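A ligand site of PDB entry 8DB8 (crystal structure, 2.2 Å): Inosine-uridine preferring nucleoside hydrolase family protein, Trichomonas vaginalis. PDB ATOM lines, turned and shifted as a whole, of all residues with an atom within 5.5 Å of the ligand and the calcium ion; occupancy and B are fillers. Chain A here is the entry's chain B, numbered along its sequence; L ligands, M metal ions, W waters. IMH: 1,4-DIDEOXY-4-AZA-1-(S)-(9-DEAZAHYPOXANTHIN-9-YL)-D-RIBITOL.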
ATOM      1  N   THR A   7      11.854 -21.116 -32.148  1.00  0.00           N
ATOM      2  CA  THR A   7      10.882 -20.614 -31.203  1.00  0.00           C
ATOM      3  C   THR A   7      10.846 -19.097 -31.204  1.00  0.00           C
ATOM      4  O   THR A   7      11.854 -18.426 -31.448  1.00  0.00           O
ATOM      5  CB  THR A   7      11.194 -21.106 -29.777  1.00  0.00           C
ATOM      6  OG1 THR A   7      10.220 -20.568 -28.866  1.00  0.00           O
ATOM      7  CG2 THR A   7      12.583 -20.648 -29.333  1.00  0.00           C
ATOM      8  N   ASP A   8       9.655 -18.548 -30.942  1.00  0.00           N
ATOM      9  CA  ASP A   8       9.498 -17.141 -30.589  1.00  0.00           C
ATOM     10  C   ASP A   8       9.212 -17.037 -29.097  1.00  0.00           C
ATOM     11  O   ASP A   8       8.240 -16.411 -28.655  1.00  0.00           O
ATOM     12  CB  ASP A   8       8.405 -16.498 -31.415  1.00  0.00           C
ATOM     13  CG  ASP A   8       7.057 -17.163 -31.242  1.00  0.00           C
ATOM     14  OD1 ASP A   8       7.013 -18.320 -30.777  1.00  0.00           O
ATOM     15  OD2 ASP A   8       6.032 -16.527 -31.562  1.00  0.00           O
ATOM     16  N   GLY A  10       7.635 -17.504 -26.318  1.00  0.00           N
ATOM     17  CA  GLY A  10       6.636 -17.012 -25.423  1.00  0.00           C
ATOM     18  C   GLY A  10       6.431 -17.965 -24.263  1.00  0.00           C
ATOM     19  O   GLY A  10       7.266 -18.813 -23.960  1.00  0.00           O
ATOM     20  N   ASP A  12       4.128 -20.481 -23.657  1.00  0.00           N
ATOM     21  CA  ASP A  12       3.988 -21.906 -23.935  1.00  0.00           C
ATOM     22  C   ASP A  12       5.226 -22.470 -24.633  1.00  0.00           C
ATOM     23  O   ASP A  12       5.540 -23.653 -24.451  1.00  0.00           O
ATOM     24  CB  ASP A  12       2.721 -22.161 -24.754  1.00  0.00           C
ATOM     25  CG  ASP A  12       2.777 -21.565 -26.142  1.00  0.00           C
ATOM     26  OD1 ASP A  12       3.370 -20.482 -26.305  1.00  0.00           O
ATOM     27  OD2 ASP A  12       2.227 -22.203 -27.075  1.00  0.00           O
ATOM     28  N   ASP A  13       5.941 -21.646 -25.403  1.00  0.00           N
ATOM     29  CA  ASP A  13       7.224 -22.069 -25.958  1.00  0.00           C
ATOM     30  C   ASP A  13       8.149 -22.575 -24.864  1.00  0.00           C
ATOM     31  O   ASP A  13       8.749 -23.663 -24.978  1.00  0.00           O
ATOM     32  CB  ASP A  13       7.922 -20.912 -26.685  1.00  0.00           C
ATOM     33  CG  ASP A  13       7.095 -20.296 -27.788  1.00  0.00           C
ATOM     34  OD1 ASP A  13       6.137 -19.554 -27.487  1.00  0.00           O
ATOM     35  OD2 ASP A  13       7.431 -20.531 -28.973  1.00  0.00           O
ATOM     36  N   ASN A  37       5.568 -13.877 -30.958  1.00  0.00           N
ATOM     37  CA  ASN A  37       4.929 -13.502 -29.706  1.00  0.00           C
ATOM     38  C   ASN A  37       5.487 -12.176 -29.200  1.00  0.00           C
ATOM     39  O   ASN A  37       4.734 -11.241 -28.902  1.00  0.00           O
ATOM     40  CB  ASN A  37       5.148 -14.607 -28.661  1.00  0.00           C
ATOM     41  CG  ASN A  37       4.276 -15.821 -28.915  1.00  0.00           C
ATOM     42  OD1 ASN A  37       3.187 -15.724 -29.498  1.00  0.00           O
ATOM     43  ND2 ASN A  37       4.751 -16.988 -28.469  1.00  0.00           N
ATOM     44  N   ILE A  76       2.232  -9.565 -29.988  1.00  0.00           N
ATOM     45  CA  ILE A  76       1.009  -9.678 -29.197  1.00  0.00           C
ATOM     46  C   ILE A  76       1.337  -9.526 -27.713  1.00  0.00           C
ATOM     47  O   ILE A  76       1.171 -10.491 -26.942  1.00  0.00           O
ATOM     48  CB  ILE A  76       0.272 -10.987 -29.486  1.00  0.00           C
ATOM     49  CG1 ILE A  76       1.227 -12.189 -29.412  1.00  0.00           C
ATOM     50  CG2 ILE A  76      -0.382 -10.948 -30.865  1.00  0.00           C
ATOM     51  CD1 ILE A  76       0.549 -13.535 -29.643  1.00  0.00           C
ATOM     52  N   ILE A  79      -0.984 -10.757 -24.834  1.00  0.00           N
ATOM     53  CA  ILE A  79      -1.190 -12.185 -24.652  1.00  0.00           C
ATOM     54  C   ILE A  79      -0.041 -12.818 -23.891  1.00  0.00           C
ATOM     55  O   ILE A  79      -0.243 -13.508 -22.877  1.00  0.00           O
ATOM     56  CB  ILE A  79      -1.412 -12.902 -26.006  1.00  0.00           C
ATOM     57  CG1 ILE A  79      -2.681 -12.381 -26.687  1.00  0.00           C
ATOM     58  CG2 ILE A  79      -1.485 -14.410 -25.815  1.00  0.00           C
ATOM     59  CD1 ILE A  79      -2.972 -13.037 -28.016  1.00  0.00           C
ATOM     60  N   HIS A  80       1.187 -12.604 -24.347  1.00  0.00           N
ATOM     61  CA  HIS A  80       2.373 -13.153 -23.704  1.00  0.00           C
ATOM     62  C   HIS A  80       3.127 -12.122 -22.869  1.00  0.00           C
ATOM     63  O   HIS A  80       4.204 -12.423 -22.366  1.00  0.00           O
ATOM     64  CB  HIS A  80       3.310 -13.756 -24.752  1.00  0.00           C
ATOM     65  CG  HIS A  80       2.808 -15.047 -25.326  1.00  0.00           C
ATOM     66  ND1 HIS A  80       3.415 -16.261 -25.081  1.00  0.00           N
ATOM     67  CD2 HIS A  80       1.775 -15.307 -26.151  1.00  0.00           C
ATOM     68  CE1 HIS A  80       2.760 -17.216 -25.716  1.00  0.00           C
ATOM     69  NE2 HIS A  80       1.765 -16.660 -26.380  1.00  0.00           N
ATOM     70  N   LEU A 125       8.214 -23.919 -33.408  1.00  0.00           N
ATOM     71  CA  LEU A 125       7.208 -23.434 -32.478  1.00  0.00           C
ATOM     72  C   LEU A 125       6.804 -21.997 -32.736  1.00  0.00           C
ATOM     73  O   LEU A 125       6.308 -21.321 -31.833  1.00  0.00           O
ATOM     74  CB  LEU A 125       7.713 -23.566 -31.041  1.00  0.00           C
ATOM     75  CG  LEU A 125       8.071 -24.970 -30.543  1.00  0.00           C
ATOM     76  CD1 LEU A 125       8.604 -24.903 -29.118  1.00  0.00           C
ATOM     77  CD2 LEU A 125       6.871 -25.888 -30.626  1.00  0.00           C
ATOM     78  N   ALA A 126       6.994 -21.506 -33.954  1.00  0.00           N
ATOM     79  CA  ALA A 126       6.951 -20.070 -34.212  1.00  0.00           C
ATOM     80  C   ALA A 126       6.731 -19.854 -35.698  1.00  0.00           C
ATOM     81  O   ALA A 126       6.744 -20.825 -36.483  1.00  0.00           O
ATOM     82  CB  ALA A 126       8.238 -19.390 -33.734  1.00  0.00           C
ATOM     83  N   MET A 151       4.277 -26.632 -34.827  1.00  0.00           N
ATOM     84  CA  MET A 151       3.088 -26.034 -34.227  1.00  0.00           C
ATOM     85  C   MET A 151       2.592 -24.936 -35.160  1.00  0.00           C
ATOM     86  O   MET A 151       3.316 -23.974 -35.442  1.00  0.00           O
ATOM     87  CB  MET A 151       3.420 -25.463 -32.843  1.00  0.00           C
ATOM     88  CG  MET A 151       2.252 -25.281 -31.869  1.00  0.00           C
ATOM     89  SD  MET A 151       0.788 -24.444 -32.497  1.00  0.00           S
ATOM     90  CE  MET A 151       1.451 -22.847 -32.885  1.00  0.00           C
ATOM     91  N   ASN A 160      -6.985 -18.251 -34.046  1.00  0.00           N
ATOM     92  CA  ASN A 160      -7.006 -17.410 -32.861  1.00  0.00           C
ATOM     93  C   ASN A 160      -6.816 -15.934 -33.209  1.00  0.00           C
ATOM     94  O   ASN A 160      -7.695 -15.115 -32.936  1.00  0.00           O
ATOM     95  CB  ASN A 160      -5.942 -17.861 -31.850  1.00  0.00           C
ATOM     96  CG  ASN A 160      -4.644 -18.291 -32.515  1.00  0.00           C
ATOM     97  OD1 ASN A 160      -4.374 -17.924 -33.665  1.00  0.00           O
ATOM     98  ND2 ASN A 160      -3.838 -19.065 -31.803  1.00  0.00           N
ATOM     99  N   ILE A 161      -5.697 -15.588 -33.839  1.00  0.00           N
ATOM    100  CA  ILE A 161      -5.396 -14.188 -34.115  1.00  0.00           C
ATOM    101  C   ILE A 161      -6.377 -13.612 -35.132  1.00  0.00           C
ATOM    102  O   ILE A 161      -6.728 -12.431 -35.070  1.00  0.00           O
ATOM    103  CB  ILE A 161      -3.922 -14.045 -34.561  1.00  0.00           C
ATOM    104  CG1 ILE A 161      -3.450 -12.603 -34.361  1.00  0.00           C
ATOM    105  CG2 ILE A 161      -3.716 -14.507 -35.999  1.00  0.00           C
ATOM    106  CD1 ILE A 161      -3.216 -12.252 -32.910  1.00  0.00           C
ATOM    107  N   GLU A 166      -4.336 -19.446 -37.706  1.00  0.00           N
ATOM    108  CA  GLU A 166      -3.500 -19.620 -36.537  1.00  0.00           C
ATOM    109  C   GLU A 166      -2.324 -18.658 -36.607  1.00  0.00           C
ATOM    110  O   GLU A 166      -1.856 -18.290 -37.684  1.00  0.00           O
ATOM    111  CB  GLU A 166      -3.022 -21.079 -36.449  1.00  0.00           C
ATOM    112  CG  GLU A 166      -2.078 -21.379 -35.288  1.00  0.00           C
ATOM    113  CD  GLU A 166      -0.640 -21.043 -35.619  1.00  0.00           C
ATOM    114  OE1 GLU A 166      -0.266 -21.121 -36.804  1.00  0.00           O
ATOM    115  OE2 GLU A 166       0.112 -20.647 -34.691  1.00  0.00           O
ATOM    116  N   PHE A 167      -1.837 -18.247 -35.429  1.00  0.00           N
ATOM    117  CA  PHE A 167      -0.937 -17.101 -35.334  1.00  0.00           C
ATOM    118  C   PHE A 167       0.352 -17.314 -36.120  1.00  0.00           C
ATOM    119  O   PHE A 167       0.747 -16.466 -36.928  1.00  0.00           O
ATOM    120  CB  PHE A 167      -0.628 -16.800 -33.868  1.00  0.00           C
ATOM    121  CG  PHE A 167       0.503 -15.817 -33.684  1.00  0.00           C
ATOM    122  CD1 PHE A 167       0.267 -14.460 -33.822  1.00  0.00           C
ATOM    123  CD2 PHE A 167       1.774 -16.246 -33.397  1.00  0.00           C
ATOM    124  CE1 PHE A 167       1.296 -13.544 -33.672  1.00  0.00           C
ATOM    125  CE2 PHE A 167       2.812 -15.341 -33.245  1.00  0.00           C
ATOM    126  CZ  PHE A 167       2.569 -13.987 -33.371  1.00  0.00           C
ATOM    127  N   ASN A 168       1.051 -18.428 -35.865  1.00  0.00           N
ATOM    128  CA  ASN A 168       2.374 -18.622 -36.461  1.00  0.00           C
ATOM    129  C   ASN A 168       2.310 -18.599 -37.985  1.00  0.00           C
ATOM    130  O   ASN A 168       3.170 -18.004 -38.640  1.00  0.00           O
ATOM    131  CB  ASN A 168       2.967 -19.945 -35.983  1.00  0.00           C
ATOM    132  CG  ASN A 168       3.436 -19.885 -34.547  1.00  0.00           C
ATOM    133  OD1 ASN A 168       3.466 -18.819 -33.940  1.00  0.00           O
ATOM    134  ND2 ASN A 168       3.810 -21.037 -34.006  1.00  0.00           N
ATOM    135  N   TRP A 193      -3.631 -25.341 -34.025  1.00  0.00           N
ATOM    136  CA  TRP A 193      -4.480 -24.685 -33.031  1.00  0.00           C
ATOM    137  C   TRP A 193      -5.763 -25.472 -32.814  1.00  0.00           C
ATOM    138  O   TRP A 193      -6.379 -25.372 -31.748  1.00  0.00           O
ATOM    139  CB  TRP A 193      -4.790 -23.258 -33.479  1.00  0.00           C
ATOM    140  CG  TRP A 193      -5.566 -22.453 -32.466  1.00  0.00           C
ATOM    141  CD1 TRP A 193      -6.835 -21.974 -32.614  1.00  0.00           C
ATOM    142  CD2 TRP A 193      -5.123 -22.020 -31.175  1.00  0.00           C
ATOM    143  NE1 TRP A 193      -7.213 -21.276 -31.496  1.00  0.00           N
ATOM    144  CE2 TRP A 193      -6.181 -21.291 -30.593  1.00  0.00           C
ATOM    145  CE3 TRP A 193      -3.932 -22.171 -30.453  1.00  0.00           C
ATOM    146  CZ2 TRP A 193      -6.083 -20.716 -29.319  1.00  0.00           C
ATOM    147  CZ3 TRP A 193      -3.847 -21.608 -29.189  1.00  0.00           C
ATOM    148  CH2 TRP A 193      -4.910 -20.896 -28.640  1.00  0.00           C
ATOM    149  N   ILE A 227      -1.357 -15.390 -19.216  1.00  0.00           N
ATOM    150  CA  ILE A 227      -2.038 -15.958 -20.385  1.00  0.00           C
ATOM    151  C   ILE A 227      -3.224 -16.817 -19.963  1.00  0.00           C
ATOM    152  O   ILE A 227      -4.188 -16.948 -20.719  1.00  0.00           O
ATOM    153  CB  ILE A 227      -1.046 -16.730 -21.265  1.00  0.00           C
ATOM    154  CG1 ILE A 227      -1.443 -16.624 -22.737  1.00  0.00           C
ATOM    155  CG2 ILE A 227      -0.960 -18.187 -20.845  1.00  0.00           C
ATOM    156  CD1 ILE A 227      -0.484 -17.324 -23.670  1.00  0.00           C
ATOM    157  N   PHE A 230      -5.852 -14.246 -19.471  1.00  0.00           N
ATOM    158  CA  PHE A 230      -6.274 -13.722 -20.769  1.00  0.00           C
ATOM    159  C   PHE A 230      -7.197 -14.693 -21.488  1.00  0.00           C
ATOM    160  O   PHE A 230      -8.076 -14.257 -22.254  1.00  0.00           O
ATOM    161  CB  PHE A 230      -5.044 -13.418 -21.636  1.00  0.00           C
ATOM    162  CG  PHE A 230      -5.323 -13.449 -23.114  1.00  0.00           C
ATOM    163  CD1 PHE A 230      -5.029 -14.569 -23.871  1.00  0.00           C
ATOM    164  CD2 PHE A 230      -5.892 -12.343 -23.745  1.00  0.00           C
ATOM    165  CE1 PHE A 230      -5.296 -14.598 -25.232  1.00  0.00           C
ATOM    166  CE2 PHE A 230      -6.152 -12.366 -25.102  1.00  0.00           C
ATOM    167  CZ  PHE A 230      -5.857 -13.500 -25.844  1.00  0.00           C
ATOM    168  N   ASP A 231      -7.037 -15.985 -21.262  1.00  0.00           N
ATOM    169  CA  ASP A 231      -7.837 -16.995 -21.943  1.00  0.00           C
ATOM    170  C   ASP A 231      -9.128 -17.320 -21.209  1.00  0.00           C
ATOM    171  O   ASP A 231      -9.939 -18.103 -21.727  1.00  0.00           O
ATOM    172  CB  ASP A 231      -7.016 -18.279 -22.116  1.00  0.00           C
ATOM    173  CG  ASP A 231      -6.560 -18.481 -23.550  1.00  0.00           C
ATOM    174  OD1 ASP A 231      -7.179 -17.908 -24.467  1.00  0.00           O
ATOM    175  OD2 ASP A 231      -5.568 -19.210 -23.753  1.00  0.00           O
ATOM    176  N   CYS A 236      -4.687 -23.509 -23.558  1.00  0.00           N
ATOM    177  CA  CYS A 236      -4.532 -24.155 -24.851  1.00  0.00           C
ATOM    178  C   CYS A 236      -3.048 -24.444 -25.067  1.00  0.00           C
ATOM    179  O   CYS A 236      -2.339 -23.633 -25.677  1.00  0.00           O
ATOM    180  CB  CYS A 236      -5.093 -23.301 -25.987  1.00  0.00           C
ATOM    181  SG  CYS A 236      -6.660 -22.484 -25.579  1.00  0.00           S
ATOM    182  N   ALA A 238      -0.558 -25.079 -26.848  1.00  0.00           N
ATOM    183  CA  ALA A 238      -0.227 -25.320 -28.254  1.00  0.00           C
ATOM    184  C   ALA A 238       1.207 -25.798 -28.418  1.00  0.00           C
ATOM    185  O   ALA A 238       1.455 -26.891 -28.929  1.00  0.00           O
ATOM    186  CB  ALA A 238      -0.467 -24.043 -29.064  1.00  0.00           C
ATOM    187  N   ASP A 239       2.185 -24.977 -28.003  1.00  0.00           N
ATOM    188  CA  ASP A 239       3.585 -25.383 -28.161  1.00  0.00           C
ATOM    189  C   ASP A 239       3.927 -26.601 -27.312  1.00  0.00           C
ATOM    190  O   ASP A 239       4.608 -27.508 -27.820  1.00  0.00           O
ATOM    191  CB  ASP A 239       4.509 -24.196 -27.867  1.00  0.00           C
ATOM    192  CG  ASP A 239       4.584 -23.219 -29.022  1.00  0.00           C
ATOM    193  OD1 ASP A 239       3.932 -23.432 -30.058  1.00  0.00           O
ATOM    194  OD2 ASP A 239       5.294 -22.205 -28.892  1.00  0.00           O
HETATM  195  O5' IMH L   1      -1.153 -19.843 -32.436  1.00  0.00           O
HETATM  196  C5' IMH L   1      -0.427 -20.340 -31.348  1.00  0.00           C
HETATM  197  C4' IMH L   1       0.963 -19.764 -31.342  1.00  0.00           C
HETATM  198  N4' IMH L   1       0.970 -18.466 -31.070  1.00  0.00           N
HETATM  199  C3' IMH L   1       1.899 -20.519 -30.175  1.00  0.00           C
HETATM  200  O3' IMH L   1       3.197 -20.861 -30.778  1.00  0.00           O
HETATM  201  C2' IMH L   1       1.990 -19.735 -29.173  1.00  0.00           C
HETATM  202  O2' IMH L   1       3.382 -19.406 -28.791  1.00  0.00           O
HETATM  203  C1' IMH L   1       1.196 -18.379 -29.560  1.00  0.00           C
HETATM  204  C9  IMH L   1      -0.032 -18.323 -28.883  1.00  0.00           C
HETATM  205  C8  IMH L   1      -0.525 -19.021 -27.814  1.00  0.00           C
HETATM  206  N7  IMH L   1      -1.771 -18.594 -27.586  1.00  0.00           N
HETATM  207  C5  IMH L   1      -2.079 -17.628 -28.524  1.00  0.00           C
HETATM  208  C6  IMH L   1      -3.211 -16.884 -28.740  1.00  0.00           C
HETATM  209  O6  IMH L   1      -4.453 -16.831 -28.080  1.00  0.00           O
HETATM  210  N1  IMH L   1      -3.250 -16.000 -29.725  1.00  0.00           N
HETATM  211  C2  IMH L   1      -2.173 -15.836 -30.538  1.00  0.00           C
HETATM  212  N3  IMH L   1      -1.055 -16.574 -30.328  1.00  0.00           N
HETATM  213  C4  IMH L   1      -1.008 -17.466 -29.325  1.00  0.00           C
HETATM  214 CA    CA M   1       5.332 -20.068 -30.057  1.00  0.00          CA
HETATM  215  O   HOH W   1       4.166 -18.500 -31.535  1.00  0.00           O
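Residues that only touch the calcium ion: Asn 37 (3.5 Å). The nearest printed residue that does not touch the calcium ion is Asp 12 (4.3 Å).
The calcium ion is bound by the backbone carbonyl oxygen (O) of Leu 125, an oxygen (O3') of the ligand, the side-chain carboxylate (OD2) of Asp 13, an oxygen (O2') of the ligand, the side-chain carboxylate (OD2) of Asp 239, water W1, the side-chain carboxylate (OD1) of Asp 8 and the side-chain carboxylate (OD1) of Asp 13. The calcium ion has eight donor atoms within binding distance.
The backbone NH of Asn 168 is in hydrogen-bond range of the side-chain carboxylate of Glu 166, at 2.7 Å. O of Asn 37 lies within hydrogen-bond range of N of Ile 76. The side-chain amide nitrogen of Asn 168 lies close to the backbone carbonyl oxygen of Leu 125, 3.3 Å away. OD1 of Asn 160 is in hydrogen-bond range of N of Phe 167, 3.1 Å away. The side-chain carboxylate of Asp 13 sits close to the side-chain amide nitrogen of Asn 37 (3.1 Å). N of Gly 10 lies close to OD1 of Asp 13, 2.8 Å away. N of Asn 37 sits at hydrogen-bond distance from OD2 of Asp 8, 2.8 Å away. The backbone NH of Asp 239 sits at hydrogen-bond distance from the side-chain carboxylate of Asp 12, at 2.9 Å.
An oxygen (O5') of the ligand lies close to the backbone NH of Phe 167. The side-chain amide nitrogen (ND2) of Asn 168 sits close to an oxygen (O3') of the ligand (3.3 Å). The side-chain amide nitrogen (ND2) of Asn 160 lies within hydrogen-bond range of an oxygen (O5') of the ligand, at 2.9 Å. OE2 of Glu 166 lies within hydrogen-bond range of O5' of the ligand (2.7 Å). The side-chain amide nitrogen (ND2) of Asn 37 lies close to an oxygen (O2') of the ligand (2.8 Å). The side-chain carboxylate (OD1) of Asp 12 sits close to an oxygen (O2') of the ligand (2.7 Å).
Water W1 lies within hydrogen-bond range of the side-chain amide oxygen (OD1) of Asn 168 (2.5 Å), the side-chain carboxylate (OD2) of Asp 8 (2.7 Å), a nitrogen (N4') of the ligand (3.2 Å) and the side-chain amide nitrogen (ND2) of Asn 37 (3.5 Å).
Merely in contact with the ligand: Ile 76, Ile 79, His 80, Met 151, Trp 193 and Phe 230. Hydrophobic or aromatic side chains within 4 Å of the ligand: Ile 76, Ile 79, His 80, Met 151, Phe 167, Trp 193 and Phe 230. Along chain A the residues within 4 Å of the ligand span positions 12 to 239.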
